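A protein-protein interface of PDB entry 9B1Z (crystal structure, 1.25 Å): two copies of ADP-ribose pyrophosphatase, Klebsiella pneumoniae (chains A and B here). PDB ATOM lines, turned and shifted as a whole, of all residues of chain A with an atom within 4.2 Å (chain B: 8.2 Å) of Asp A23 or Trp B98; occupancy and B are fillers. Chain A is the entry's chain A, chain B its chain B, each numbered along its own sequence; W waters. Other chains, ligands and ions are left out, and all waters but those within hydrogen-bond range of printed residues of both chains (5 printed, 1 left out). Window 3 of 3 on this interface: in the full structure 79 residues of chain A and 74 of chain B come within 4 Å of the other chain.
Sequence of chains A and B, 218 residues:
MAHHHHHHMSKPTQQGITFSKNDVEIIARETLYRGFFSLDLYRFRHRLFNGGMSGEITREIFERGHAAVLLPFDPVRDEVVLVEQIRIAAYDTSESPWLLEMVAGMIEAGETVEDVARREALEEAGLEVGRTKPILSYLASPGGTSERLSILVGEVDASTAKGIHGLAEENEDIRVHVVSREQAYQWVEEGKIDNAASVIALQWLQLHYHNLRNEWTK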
ATOM      1  N   PHE A  19     -20.663  -2.032  11.750  1.00  0.00           N
ATOM      2  CA  PHE A  19     -20.483  -3.475  11.667  1.00  0.00           C
ATOM      3  C   PHE A  19     -19.226  -3.852  10.877  1.00  0.00           C
ATOM      4  O   PHE A  19     -18.665  -3.039  10.137  1.00  0.00           O
ATOM      5  CB  PHE A  19     -21.715  -4.038  10.980  1.00  0.00           C
ATOM      6  CG  PHE A  19     -22.975  -3.919  11.779  1.00  0.00           C
ATOM      7  CD1 PHE A  19     -23.020  -4.344  13.091  1.00  0.00           C
ATOM      8  CD2 PHE A  19     -24.129  -3.414  11.202  1.00  0.00           C
ATOM      9  CE1 PHE A  19     -24.204  -4.275  13.809  1.00  0.00           C
ATOM     10  CE2 PHE A  19     -25.298  -3.347  11.903  1.00  0.00           C
ATOM     11  CZ  PHE A  19     -25.344  -3.771  13.204  1.00  0.00           C
ATOM     12  N   SER A  20     -18.783  -5.105  11.048  1.00  0.00           N
ATOM     13  CA  SER A  20     -17.582  -5.646  10.409  1.00  0.00           C
ATOM     14  C   SER A  20     -17.923  -6.942   9.674  1.00  0.00           C
ATOM     15  O   SER A  20     -19.066  -7.406   9.686  1.00  0.00           O
ATOM     16  CB  SER A  20     -16.496  -5.929  11.458  1.00  0.00           C
ATOM     17  OG  SER A  20     -16.792  -7.113  12.180  1.00  0.00           O
ATOM     18  N   LYS A  21     -16.902  -7.573   9.085  1.00  0.00           N
ATOM     19  CA  LYS A  21     -17.095  -8.876   8.448  1.00  0.00           C
ATOM     20  C   LYS A  21     -17.479  -9.969   9.441  1.00  0.00           C
ATOM     21  O   LYS A  21     -18.092 -10.970   9.047  1.00  0.00           O
ATOM     22  CB  LYS A  21     -15.832  -9.256   7.684  1.00  0.00           C
ATOM     23  CG  LYS A  21     -15.685  -8.411   6.450  1.00  0.00           C
ATOM     24  CD  LYS A  21     -14.429  -8.709   5.674  1.00  0.00           C
ATOM     25  CE  LYS A  21     -14.468  -7.942   4.381  1.00  0.00           C
ATOM     26  NZ  LYS A  21     -13.189  -8.003   3.662  1.00  0.00           N
ATOM     27  N   ASN A  22     -17.185  -9.784  10.724  1.00  0.00           N
ATOM     28  CA  ASN A  22     -17.664 -10.736  11.713  1.00  0.00           C
ATOM     29  C   ASN A  22     -19.184 -10.712  11.864  1.00  0.00           C
ATOM     30  O   ASN A  22     -19.754 -11.679  12.386  1.00  0.00           O
ATOM     31  CB  ASN A  22     -16.997 -10.476  13.053  1.00  0.00           C
ATOM     32  CG  ASN A  22     -17.178 -11.626  14.003  1.00  0.00           C
ATOM     33  OD1 ASN A  22     -16.805 -12.759  13.697  1.00  0.00           O
ATOM     34  ND2 ASN A  22     -17.759 -11.353  15.160  1.00  0.00           N
ATOM     35  N   ASP A  23     -19.840  -9.646  11.397  1.00  0.00           N
ATOM     36  CA  ASP A  23     -21.288  -9.491  11.440  1.00  0.00           C
ATOM     37  C   ASP A  23     -21.980 -10.021  10.197  1.00  0.00           C
ATOM     38  O   ASP A  23     -23.182  -9.792  10.025  1.00  0.00           O
ATOM     39  CB  ASP A  23     -21.621  -8.015  11.641  1.00  0.00           C
ATOM     40  CG  ASP A  23     -21.108  -7.491  12.955  1.00  0.00           C
ATOM     41  OD1 ASP A  23     -21.549  -8.045  13.969  1.00  0.00           O
ATOM     42  OD2 ASP A  23     -20.274  -6.559  12.965  1.00  0.00           O
ATOM     43  N   VAL A  24     -21.251 -10.737   9.347  1.00  0.00           N
ATOM     44  CA  VAL A  24     -21.773 -11.344   8.136  1.00  0.00           C
ATOM     45  C   VAL A  24     -21.476 -12.833   8.167  1.00  0.00           C
ATOM     46  O   VAL A  24     -20.374 -13.252   8.546  1.00  0.00           O
ATOM     47  CB  VAL A  24     -21.079 -10.738   6.903  1.00  0.00           C
ATOM     48  CG1 VAL A  24     -21.648 -11.327   5.615  1.00  0.00           C
ATOM     49  CG2 VAL A  24     -21.205  -9.247   6.913  1.00  0.00           C
ATOM     50  N   HIS A  46     -26.765 -11.312   7.753  1.00  0.00           N
ATOM     51  CA  HIS A  46     -25.997 -10.203   8.308  1.00  0.00           C
ATOM     52  C   HIS A  46     -26.713  -9.619   9.512  1.00  0.00           C
ATOM     53  O   HIS A  46     -27.932  -9.719   9.636  1.00  0.00           O
ATOM     54  CB  HIS A  46     -25.782  -9.108   7.253  1.00  0.00           C
ATOM     55  CG  HIS A  46     -27.056  -8.518   6.746  1.00  0.00           C
ATOM     56  ND1 HIS A  46     -27.685  -7.458   7.359  1.00  0.00           N
ATOM     57  CD2 HIS A  46     -27.807  -8.823   5.662  1.00  0.00           C
ATOM     58  CE1 HIS A  46     -28.783  -7.154   6.690  1.00  0.00           C
ATOM     59  NE2 HIS A  46     -28.878  -7.968   5.653  1.00  0.00           N
ATOM     60  N   ARG A  47     -25.943  -8.976  10.382  1.00  0.00           N
ATOM     61  CA  ARG A  47     -26.531  -8.359  11.562  1.00  0.00           C
ATOM     62  C   ARG A  47     -27.395  -7.166  11.165  1.00  0.00           C
ATOM     63  O   ARG A  47     -27.136  -6.470  10.169  1.00  0.00           O
ATOM     64  CB  ARG A  47     -25.432  -7.984  12.564  1.00  0.00           C
ATOM     65  CG  ARG A  47     -25.933  -7.497  13.912  1.00  0.00           C
ATOM     66  CD  ARG A  47     -24.878  -7.703  15.039  1.00  0.00           C
ATOM     67  NE  ARG A  47     -25.061  -8.996  15.699  1.00  0.00           N
ATOM     68  CZ  ARG A  47     -24.459 -10.136  15.363  1.00  0.00           C
ATOM     69  NH1 ARG A  47     -23.436 -10.175  14.505  1.00  0.00           N
ATOM     70  NH2 ARG A  47     -24.911 -11.273  15.892  1.00  0.00           N
ATOM     71  N   PHE A  49     -29.370  -3.493  12.289  1.00  0.00           N
ATOM     72  CA  PHE A  49     -29.070  -2.310  13.097  1.00  0.00           C
ATOM     73  C   PHE A  49     -29.710  -2.365  14.480  1.00  0.00           C
ATOM     74  O   PHE A  49     -29.121  -1.892  15.456  1.00  0.00           O
ATOM     75  CB  PHE A  49     -29.489  -1.037  12.364  1.00  0.00           C
ATOM     76  CG  PHE A  49     -28.586  -0.688  11.227  1.00  0.00           C
ATOM     77  CD1 PHE A  49     -27.272  -0.330  11.463  1.00  0.00           C
ATOM     78  CD2 PHE A  49     -29.034  -0.752   9.921  1.00  0.00           C
ATOM     79  CE1 PHE A  49     -26.427  -0.016  10.415  1.00  0.00           C
ATOM     80  CE2 PHE A  49     -28.187  -0.438   8.861  1.00  0.00           C
ATOM     81  CZ  PHE A  49     -26.886  -0.069   9.115  1.00  0.00           C
ATOM     82  N   MET A  53     -29.783 -11.193  13.739  1.00  0.00           N
ATOM     83  CA  MET A  53     -29.345 -11.516  12.390  1.00  0.00           C
ATOM     84  C   MET A  53     -30.525 -11.538  11.430  1.00  0.00           C
ATOM     85  O   MET A  53     -31.640 -11.929  11.789  1.00  0.00           O
ATOM     86  CB  MET A  53     -28.630 -12.871  12.346  1.00  0.00           C
ATOM     87  CG  MET A  53     -27.320 -12.905  13.088  1.00  0.00           C
ATOM     88  SD  MET A  53     -26.034 -11.806  12.503  1.00  0.00           S
ATOM     89  CE  MET A  53     -25.642 -12.589  10.961  1.00  0.00           C
ATOM     90  N   VAL B  83     -27.553   7.133   3.257  1.00  0.00           N
ATOM     91  CA  VAL B  83     -28.195   5.905   3.716  1.00  0.00           C
ATOM     92  C   VAL B  83     -27.150   4.811   3.846  1.00  0.00           C
ATOM     93  O   VAL B  83     -26.303   4.639   2.973  1.00  0.00           O
ATOM     94  CB  VAL B  83     -29.376   5.477   2.829  1.00  0.00           C
ATOM     95  CG1 VAL B  83     -30.477   6.506   2.935  1.00  0.00           C
ATOM     96  CG2 VAL B  83     -28.955   5.278   1.434  1.00  0.00           C
ATOM     97  N   GLU B  84     -27.206   4.065   4.931  1.00  0.00           N
ATOM     98  CA  GLU B  84     -26.250   3.003   5.198  1.00  0.00           C
ATOM     99  C   GLU B  84     -26.956   1.654   5.143  1.00  0.00           C
ATOM    100  O   GLU B  84     -27.968   1.447   5.820  1.00  0.00           O
ATOM    101  CB  GLU B  84     -25.615   3.173   6.576  1.00  0.00           C
ATOM    102  CG  GLU B  84     -24.509   2.171   6.857  1.00  0.00           C
ATOM    103  CD  GLU B  84     -24.001   2.235   8.275  1.00  0.00           C
ATOM    104  OE1 GLU B  84     -24.536   3.018   9.083  1.00  0.00           O
ATOM    105  OE2 GLU B  84     -23.073   1.472   8.592  1.00  0.00           O
ATOM    106  N   GLN B  85     -26.382   0.719   4.394  1.00  0.00           N
ATOM    107  CA  GLN B  85     -26.896  -0.640   4.346  1.00  0.00           C
ATOM    108  C   GLN B  85     -25.822  -1.543   3.768  1.00  0.00           C
ATOM    109  O   GLN B  85     -24.853  -1.077   3.170  1.00  0.00           O
ATOM    110  CB  GLN B  85     -28.165  -0.720   3.508  1.00  0.00           C
ATOM    111  CG  GLN B  85     -27.920  -0.481   2.039  1.00  0.00           C
ATOM    112  CD  GLN B  85     -29.196  -0.169   1.317  1.00  0.00           C
ATOM    113  OE1 GLN B  85     -29.980  -1.059   1.043  1.00  0.00           O
ATOM    114  NE2 GLN B  85     -29.432   1.109   1.041  1.00  0.00           N
ATOM    115  N   ILE B  86     -25.999  -2.847   3.965  1.00  0.00           N
ATOM    116  CA  ILE B  86     -25.014  -3.793   3.460  1.00  0.00           C
ATOM    117  C   ILE B  86     -25.134  -3.939   1.949  1.00  0.00           C
ATOM    118  O   ILE B  86     -26.235  -3.999   1.387  1.00  0.00           O
ATOM    119  CB  ILE B  86     -25.141  -5.147   4.183  1.00  0.00           C
ATOM    120  CG1 ILE B  86     -23.926  -6.021   3.861  1.00  0.00           C
ATOM    121  CG2 ILE B  86     -26.469  -5.865   3.838  1.00  0.00           C
ATOM    122  CD1 ILE B  86     -23.821  -7.258   4.723  1.00  0.00           C
ATOM    123  N   ARG B  87     -23.980  -4.005   1.291  1.00  0.00           N
ATOM    124  CA  ARG B  87     -23.856  -4.323  -0.131  1.00  0.00           C
ATOM    125  C   ARG B  87     -22.835  -5.451  -0.178  1.00  0.00           C
ATOM    126  O   ARG B  87     -21.630  -5.201  -0.124  1.00  0.00           O
ATOM    127  CB  ARG B  87     -23.395  -3.108  -0.926  1.00  0.00           C
ATOM    128  CG  ARG B  87     -24.359  -1.942  -0.890  1.00  0.00           C
ATOM    129  CD  ARG B  87     -25.688  -2.240  -1.540  1.00  0.00           C
ATOM    130  NE  ARG B  87     -26.524  -1.043  -1.506  1.00  0.00           N
ATOM    131  CZ  ARG B  87     -27.752  -0.977  -1.986  1.00  0.00           C
ATOM    132  NH1 ARG B  87     -28.349  -2.041  -2.502  1.00  0.00           N
ATOM    133  NH2 ARG B  87     -28.391   0.193  -1.970  1.00  0.00           N
ATOM    134  N   ILE B  88     -23.312  -6.694  -0.259  1.00  0.00           N
ATOM    135  CA  ILE B  88     -22.408  -7.821  -0.071  1.00  0.00           C
ATOM    136  C   ILE B  88     -21.298  -7.845  -1.115  1.00  0.00           C
ATOM    137  O   ILE B  88     -20.196  -8.330  -0.837  1.00  0.00           O
ATOM    138  CB  ILE B  88     -23.198  -9.137  -0.021  1.00  0.00           C
ATOM    139  CG1 ILE B  88     -22.358 -10.245   0.626  1.00  0.00           C
ATOM    140  CG2 ILE B  88     -23.685  -9.555  -1.401  1.00  0.00           C
ATOM    141  CD1 ILE B  88     -22.004 -10.004   2.088  1.00  0.00           C
ATOM    142  N   ALA B  90     -19.395  -5.598  -1.975  1.00  0.00           N
ATOM    143  CA  ALA B  90     -18.256  -4.845  -1.470  1.00  0.00           C
ATOM    144  C   ALA B  90     -17.312  -5.692  -0.613  1.00  0.00           C
ATOM    145  O   ALA B  90     -16.189  -5.264  -0.337  1.00  0.00           O
ATOM    146  CB  ALA B  90     -18.754  -3.670  -0.632  1.00  0.00           C
ATOM    147  N   TYR B  91     -17.735  -6.885  -0.203  1.00  0.00           N
ATOM    148  CA  TYR B  91     -17.023  -7.650   0.819  1.00  0.00           C
ATOM    149  C   TYR B  91     -15.557  -7.886   0.463  1.00  0.00           C
ATOM    150  O   TYR B  91     -14.671  -7.680   1.292  1.00  0.00           O
ATOM    151  CB  TYR B  91     -17.762  -8.968   0.998  1.00  0.00           C
ATOM    152  CG  TYR B  91     -17.280  -9.861   2.115  1.00  0.00           C
ATOM    153  CD1 TYR B  91     -16.178 -10.698   1.952  1.00  0.00           C
ATOM    154  CD2 TYR B  91     -17.968  -9.922   3.321  1.00  0.00           C
ATOM    155  CE1 TYR B  91     -15.763 -11.546   2.955  1.00  0.00           C
ATOM    156  CE2 TYR B  91     -17.555 -10.773   4.337  1.00  0.00           C
ATOM    157  CZ  TYR B  91     -16.449 -11.584   4.141  1.00  0.00           C
ATOM    158  OH  TYR B  91     -15.998 -12.452   5.111  1.00  0.00           O
ATOM    159  N   SER B  94     -13.271  -4.490   0.632  1.00  0.00           N
ATOM    160  CA  SER B  94     -13.572  -3.456   1.609  1.00  0.00           C
ATOM    161  C   SER B  94     -13.440  -4.049   3.000  1.00  0.00           C
ATOM    162  O   SER B  94     -13.649  -5.241   3.196  1.00  0.00           O
ATOM    163  CB  SER B  94     -15.006  -2.928   1.437  1.00  0.00           C
ATOM    164  OG  SER B  94     -15.281  -2.563   0.097  1.00  0.00           O
ATOM    165  N   GLU B  95     -13.088  -3.215   3.968  1.00  0.00           N
ATOM    166  CA  GLU B  95     -13.045  -3.706   5.339  1.00  0.00           C
ATOM    167  C   GLU B  95     -14.436  -4.078   5.836  1.00  0.00           C
ATOM    168  O   GLU B  95     -14.596  -5.065   6.554  1.00  0.00           O
ATOM    169  CB  GLU B  95     -12.372  -2.684   6.255  1.00  0.00           C
ATOM    170  CG  GLU B  95     -10.847  -2.752   6.218  1.00  0.00           C
ATOM    171  CD  GLU B  95     -10.181  -1.816   7.214  1.00  0.00           C
ATOM    172  OE1 GLU B  95     -10.807  -1.490   8.247  1.00  0.00           O
ATOM    173  OE2 GLU B  95      -9.028  -1.403   6.961  1.00  0.00           O
ATOM    174  N   SER B  96     -15.460  -3.328   5.433  1.00  0.00           N
ATOM    175  CA  SER B  96     -16.836  -3.639   5.785  1.00  0.00           C
ATOM    176  C   SER B  96     -17.735  -3.520   4.562  1.00  0.00           C
ATOM    177  O   SER B  96     -17.600  -2.566   3.790  1.00  0.00           O
ATOM    178  CB  SER B  96     -17.356  -2.670   6.843  1.00  0.00           C
ATOM    179  OG  SER B  96     -18.746  -2.893   7.039  1.00  0.00           O
ATOM    180  N   PRO B  97     -18.706  -4.420   4.387  1.00  0.00           N
ATOM    181  CA  PRO B  97     -19.645  -4.276   3.271  1.00  0.00           C
ATOM    182  C   PRO B  97     -20.813  -3.335   3.534  1.00  0.00           C
ATOM    183  O   PRO B  97     -21.630  -3.131   2.633  1.00  0.00           O
ATOM    184  CB  PRO B  97     -20.112  -5.710   3.040  1.00  0.00           C
ATOM    185  CG  PRO B  97     -20.086  -6.309   4.427  1.00  0.00           C
ATOM    186  CD  PRO B  97     -18.875  -5.704   5.092  1.00  0.00           C
ATOM    187  N   TRP B  98     -20.933  -2.756   4.727  1.00  0.00           N
ATOM    188  CA  TRP B  98     -21.927  -1.713   4.957  1.00  0.00           C
ATOM    189  C   TRP B  98     -21.408  -0.405   4.379  1.00  0.00           C
ATOM    190  O   TRP B  98     -20.333   0.066   4.774  1.00  0.00           O
ATOM    191  CB  TRP B  98     -22.217  -1.542   6.443  1.00  0.00           C
ATOM    192  CG  TRP B  98     -23.182  -2.548   7.004  1.00  0.00           C
ATOM    193  CD1 TRP B  98     -24.514  -2.357   7.222  1.00  0.00           C
ATOM    194  CD2 TRP B  98     -22.889  -3.883   7.447  1.00  0.00           C
ATOM    195  NE1 TRP B  98     -25.071  -3.487   7.775  1.00  0.00           N
ATOM    196  CE2 TRP B  98     -24.094  -4.438   7.909  1.00  0.00           C
ATOM    197  CE3 TRP B  98     -21.730  -4.659   7.494  1.00  0.00           C
ATOM    198  CZ2 TRP B  98     -24.171  -5.727   8.436  1.00  0.00           C
ATOM    199  CZ3 TRP B  98     -21.811  -5.952   8.006  1.00  0.00           C
ATOM    200  CH2 TRP B  98     -23.018  -6.470   8.467  1.00  0.00           C
ATOM    201  N   LEU B  99     -22.163   0.174   3.451  1.00  0.00           N
ATOM    202  CA  LEU B  99     -21.726   1.353   2.712  1.00  0.00           C
ATOM    203  C   LEU B  99     -22.636   2.538   3.003  1.00  0.00           C
ATOM    204  O   LEU B  99     -23.831   2.367   3.260  1.00  0.00           O
ATOM    205  CB  LEU B  99     -21.766   1.095   1.202  1.00  0.00           C
ATOM    206  CG  LEU B  99     -21.003  -0.110   0.664  1.00  0.00           C
ATOM    207  CD1 LEU B  99     -20.993  -0.037  -0.851  1.00  0.00           C
ATOM    208  CD2 LEU B  99     -19.591  -0.168   1.189  1.00  0.00           C
ATOM    209  N   LEU B 100     -22.049   3.738   2.943  1.00  0.00           N
ATOM    210  CA  LEU B 100     -22.778   5.000   2.993  1.00  0.00           C
ATOM    211  C   LEU B 100     -23.043   5.449   1.563  1.00  0.00           C
ATOM    212  O   LEU B 100     -22.099   5.637   0.786  1.00  0.00           O
ATOM    213  CB  LEU B 100     -21.935   6.052   3.708  1.00  0.00           C
ATOM    214  CG  LEU B 100     -21.670   5.732   5.182  1.00  0.00           C
ATOM    215  CD1 LEU B 100     -20.562   6.630   5.727  1.00  0.00           C
ATOM    216  CD2 LEU B 100     -22.926   5.900   5.997  1.00  0.00           C
ATOM    217  N   GLU B 101     -24.315   5.640   1.218  1.00  0.00           N
ATOM    218  CA  GLU B 101     -24.701   5.832  -0.170  1.00  0.00           C
ATOM    219  C   GLU B 101     -25.766   6.904  -0.346  1.00  0.00           C
ATOM    220  O   GLU B 101     -26.464   7.310   0.579  1.00  0.00           O
ATOM    221  CB  GLU B 101     -25.273   4.540  -0.757  1.00  0.00           C
ATOM    222  CG  GLU B 101     -24.283   3.399  -0.810  1.00  0.00           C
ATOM    223  CD  GLU B 101     -24.890   2.156  -1.410  1.00  0.00           C
ATOM    224  OE1 GLU B 101     -25.712   1.535  -0.738  1.00  0.00           O
ATOM    225  OE2 GLU B 101     -24.558   1.793  -2.556  1.00  0.00           O
ATOM    226  N   ASP B 173     -32.436  -3.282   5.401  1.00  0.00           N
ATOM    227  CA  ASP B 173     -32.198  -2.768   6.744  1.00  0.00           C
ATOM    228  C   ASP B 173     -31.309  -1.544   6.582  1.00  0.00           C
ATOM    229  O   ASP B 173     -30.126  -1.673   6.263  1.00  0.00           O
ATOM    230  CB  ASP B 173     -31.512  -3.837   7.589  1.00  0.00           C
ATOM    231  CG  ASP B 173     -31.324  -3.413   9.028  1.00  0.00           C
ATOM    232  OD1 ASP B 173     -32.288  -2.901   9.635  1.00  0.00           O
ATOM    233  OD2 ASP B 173     -30.216  -3.622   9.565  1.00  0.00           O
ATOM    234  N   ILE B 174     -31.869  -0.361   6.812  1.00  0.00           N
ATOM    235  CA  ILE B 174     -31.237   0.897   6.439  1.00  0.00           C
ATOM    236  C   ILE B 174     -31.104   1.772   7.669  1.00  0.00           C
ATOM    237  O   ILE B 174     -32.024   1.857   8.487  1.00  0.00           O
ATOM    238  CB  ILE B 174     -32.081   1.623   5.366  1.00  0.00           C
ATOM    239  CG1 ILE B 174     -32.110   0.786   4.084  1.00  0.00           C
ATOM    240  CG2 ILE B 174     -31.552   3.048   5.096  1.00  0.00           C
ATOM    241  CD1 ILE B 174     -33.154   1.228   3.085  1.00  0.00           C
ATOM    242  N   ARG B 175     -29.961   2.431   7.787  1.00  0.00           N
ATOM    243  CA  ARG B 175     -29.759   3.490   8.762  1.00  0.00           C
ATOM    244  C   ARG B 175     -29.537   4.798   8.014  1.00  0.00           C
ATOM    245  O   ARG B 175     -28.691   4.876   7.113  1.00  0.00           O
ATOM    246  CB  ARG B 175     -28.571   3.187   9.675  1.00  0.00           C
ATOM    247  CG  ARG B 175     -28.412   4.178  10.810  1.00  0.00           C
ATOM    248  CD  ARG B 175     -27.518   3.630  11.913  1.00  0.00           C
ATOM    249  NE  ARG B 175     -26.141   3.459  11.470  1.00  0.00           N
ATOM    250  CZ  ARG B 175     -25.154   3.020  12.239  1.00  0.00           C
ATOM    251  NH1 ARG B 175     -25.361   2.671  13.498  1.00  0.00           N
ATOM    252  NH2 ARG B 175     -23.924   2.940  11.735  1.00  0.00           N
ATOM    253  N   LYS B 192     -13.853   6.727   3.176  1.00  0.00           N
ATOM    254  CA  LYS B 192     -14.979   6.166   3.910  1.00  0.00           C
ATOM    255  C   LYS B 192     -16.256   6.129   3.081  1.00  0.00           C
ATOM    256  O   LYS B 192     -17.139   5.315   3.369  1.00  0.00           O
ATOM    257  CB  LYS B 192     -15.190   6.995   5.178  1.00  0.00           C
ATOM    258  CG  LYS B 192     -16.382   6.595   5.973  1.00  0.00           C
ATOM    259  CD  LYS B 192     -16.326   7.203   7.355  1.00  0.00           C
ATOM    260  CE  LYS B 192     -17.580   6.891   8.135  1.00  0.00           C
ATOM    261  NZ  LYS B 192     -17.739   5.412   8.391  1.00  0.00           N
ATOM    262  N   ASP B 194     -16.942   5.500  -0.805  1.00  0.00           N
ATOM    263  CA  ASP B 194     -16.118   5.032  -1.916  1.00  0.00           C
ATOM    264  C   ASP B 194     -16.911   4.209  -2.918  1.00  0.00           C
ATOM    265  O   ASP B 194     -16.366   3.297  -3.539  1.00  0.00           O
ATOM    266  CB  ASP B 194     -14.836   4.331  -1.437  1.00  0.00           C
ATOM    267  CG  ASP B 194     -15.059   2.920  -0.913  1.00  0.00           C
ATOM    268  OD1 ASP B 194     -16.210   2.531  -0.574  1.00  0.00           O
ATOM    269  OD2 ASP B 194     -14.034   2.203  -0.802  1.00  0.00           O
ATOM    270  N   ASN B 195     -18.174   4.538  -3.117  1.00  0.00           N
ATOM    271  CA  ASN B 195     -18.986   3.978  -4.185  1.00  0.00           C
ATOM    272  C   ASN B 195     -19.190   5.074  -5.229  1.00  0.00           C
ATOM    273  O   ASN B 195     -19.326   6.251  -4.885  1.00  0.00           O
ATOM    274  CB  ASN B 195     -20.323   3.432  -3.650  1.00  0.00           C
ATOM    275  CG  ASN B 195     -21.131   4.475  -2.914  1.00  0.00           C
ATOM    276  OD1 ASN B 195     -22.000   5.118  -3.488  1.00  0.00           O
ATOM    277  ND2 ASN B 195     -20.863   4.634  -1.627  1.00  0.00           N
HETATM  278  O   HOH W   1     -14.228  -6.325   8.857  1.00  0.00           O
HETATM  279  O   HOH W   2     -22.317  -0.602   9.741  1.00  0.00           O
HETATM  280  O   HOH W   3     -17.744 -12.936   7.056  1.00  0.00           O
HETATM  281  O   HOH W   4     -27.790  -4.259   8.622  1.00  0.00           O
HETATM  282  O   HOH W   5     -32.645  -3.259  12.322  1.00  0.00           O
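CE2 of Trp B98 touches CD2 of Phe A19, 3.4 Å away.
CH2 of Trp B98 touches O of Asp A23, at 3.7 Å.
Val A24 touches Ile B86 (CG2 to CD1, 3.9 Å).
Val A24 touches Ile B88 (CG1 to CD1, 3.8 Å).
Val A24 touches Trp B98 (CG2 to CZ3, 3.5 Å).
NE2 of His A46 touches CG2 of Ile B86 (3.7 Å).
His A46 touches Trp B98 (CB to CZ2, 3.9 Å).
O of Arg A47 touches CZ2 of Trp B98 (3.5 Å).
CZ of Phe A49 touches CD1 of Trp B98 (3.8 Å).
Phe A49 touches Arg B175 (CE2 to N, 3.5 Å).
Water W2 bridges the side-chain carboxylate (OE2) of Glu B84 (2.5 Å) and the backbone NH (N) of Phe A19 (3.0 Å).
Water W1 bridges the backbone carbonyl oxygen (O) of Glu B95 (2.7 Å) and the backbone NH (N) of Lys A21 (3.0 Å).
Water W3 lies within hydrogen-bond range of OH of Tyr B91 (2.7 Å), O of Lys A21 (2.8 Å) and O of Val A24 (3.0 Å).
Water W4 lies within hydrogen-bond range of the side-chain carboxylate (OD2) of Asp B173 (2.7 Å), the backbone carbonyl oxygen (O) of Arg A47 (2.8 Å), the indole nitrogen (NE1) of Trp B98 (3.0 Å) and a ring nitrogen (ND1) of His A46 (3.4 Å).
Water W5 bridges the side-chain carboxylate of Asp B173 (2.7 Å) and the backbone NH of Phe A49 (3.3 Å).
The side-chain carboxylate (OD1) of Asp A23 is in salt-bridge range of the guanidinium group (NH1) of Arg A47 (2.9 Å).
The backbone NH (N) of Trp B98 sits at hydrogen-bond distance from the side-chain hydroxyl (OG) of Ser B96, at 3.2 Å.
OE1 of Glu B84 lies within salt-bridge range of NH2 of Arg B175 (2.7 Å).
N of Ser A20 lies within hydrogen-bond range of OD2 of Asp A23 (2.8 Å).
N of Arg A47 sits at hydrogen-bond distance from SD of Met A53 (3.5 Å).
O of Ala B90 is in hydrogen-bond range of OG of Ser B94 (2.9 Å).
Of chain B, only Trp B98 (3.7 Å) comes within 4 Å of Asp A23.
Trp B98 touches just these residues of chain A: Phe A19 (3.4 Å), Ser A20 (3.5 Å), Asp A23 (3.7 Å), Val A24 (3.5 Å), His A46 (3.9 Å), Arg A47 (3.5 Å) and Phe A49 (3.8 Å).
Of chain B, only Trp B98 comes within 4 Å of Ser A20.
Of the printed residues of chain A, Ile B174 touches Phe A49.
Of the printed residues of chain A, Ile B86 touches Val A24 and His A46.
Printed residues of chain A within 4 Å of Glu B84: Phe A49 (3.6 Å).
The nearest printed residue of chain A that does not touch Trp B98 is Lys A21 (5.3 Å).
The nearest printed residue of chain A that does not touch Tyr B91 is Val A24 (4.3 Å).
The side-chain hydroxyl of Ser B96 sits at hydrogen-bond distance from the backbone carbonyl oxygen of Phe A19, at 3.1 Å.
The side-chain amino group (NZ) of Lys A21 sits at hydrogen-bond distance from the backbone carbonyl oxygen (O) of Ser B94, 2.8 Å away.
OD2 of Asp B173 sits at hydrogen-bond distance from N of Phe A49 (2.9 Å).
The backbone carbonyl oxygen (O) of Tyr B91 is in hydrogen-bond range of the side-chain amino group (NZ) of Lys A21 (2.8 Å).
Of the 10 printed residues of chain A, 8 touch a printed residue of chain B.
Along chain B the printed residues that touch a printed residue of chain A span positions 84 to 175.
Among the printed residues, 18 pairs touch across the chains.
No position is printed for both chains.
Of the 18 pairs that touch across the chains among the printed residues, none has its exchanged pair printed and touching as well.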
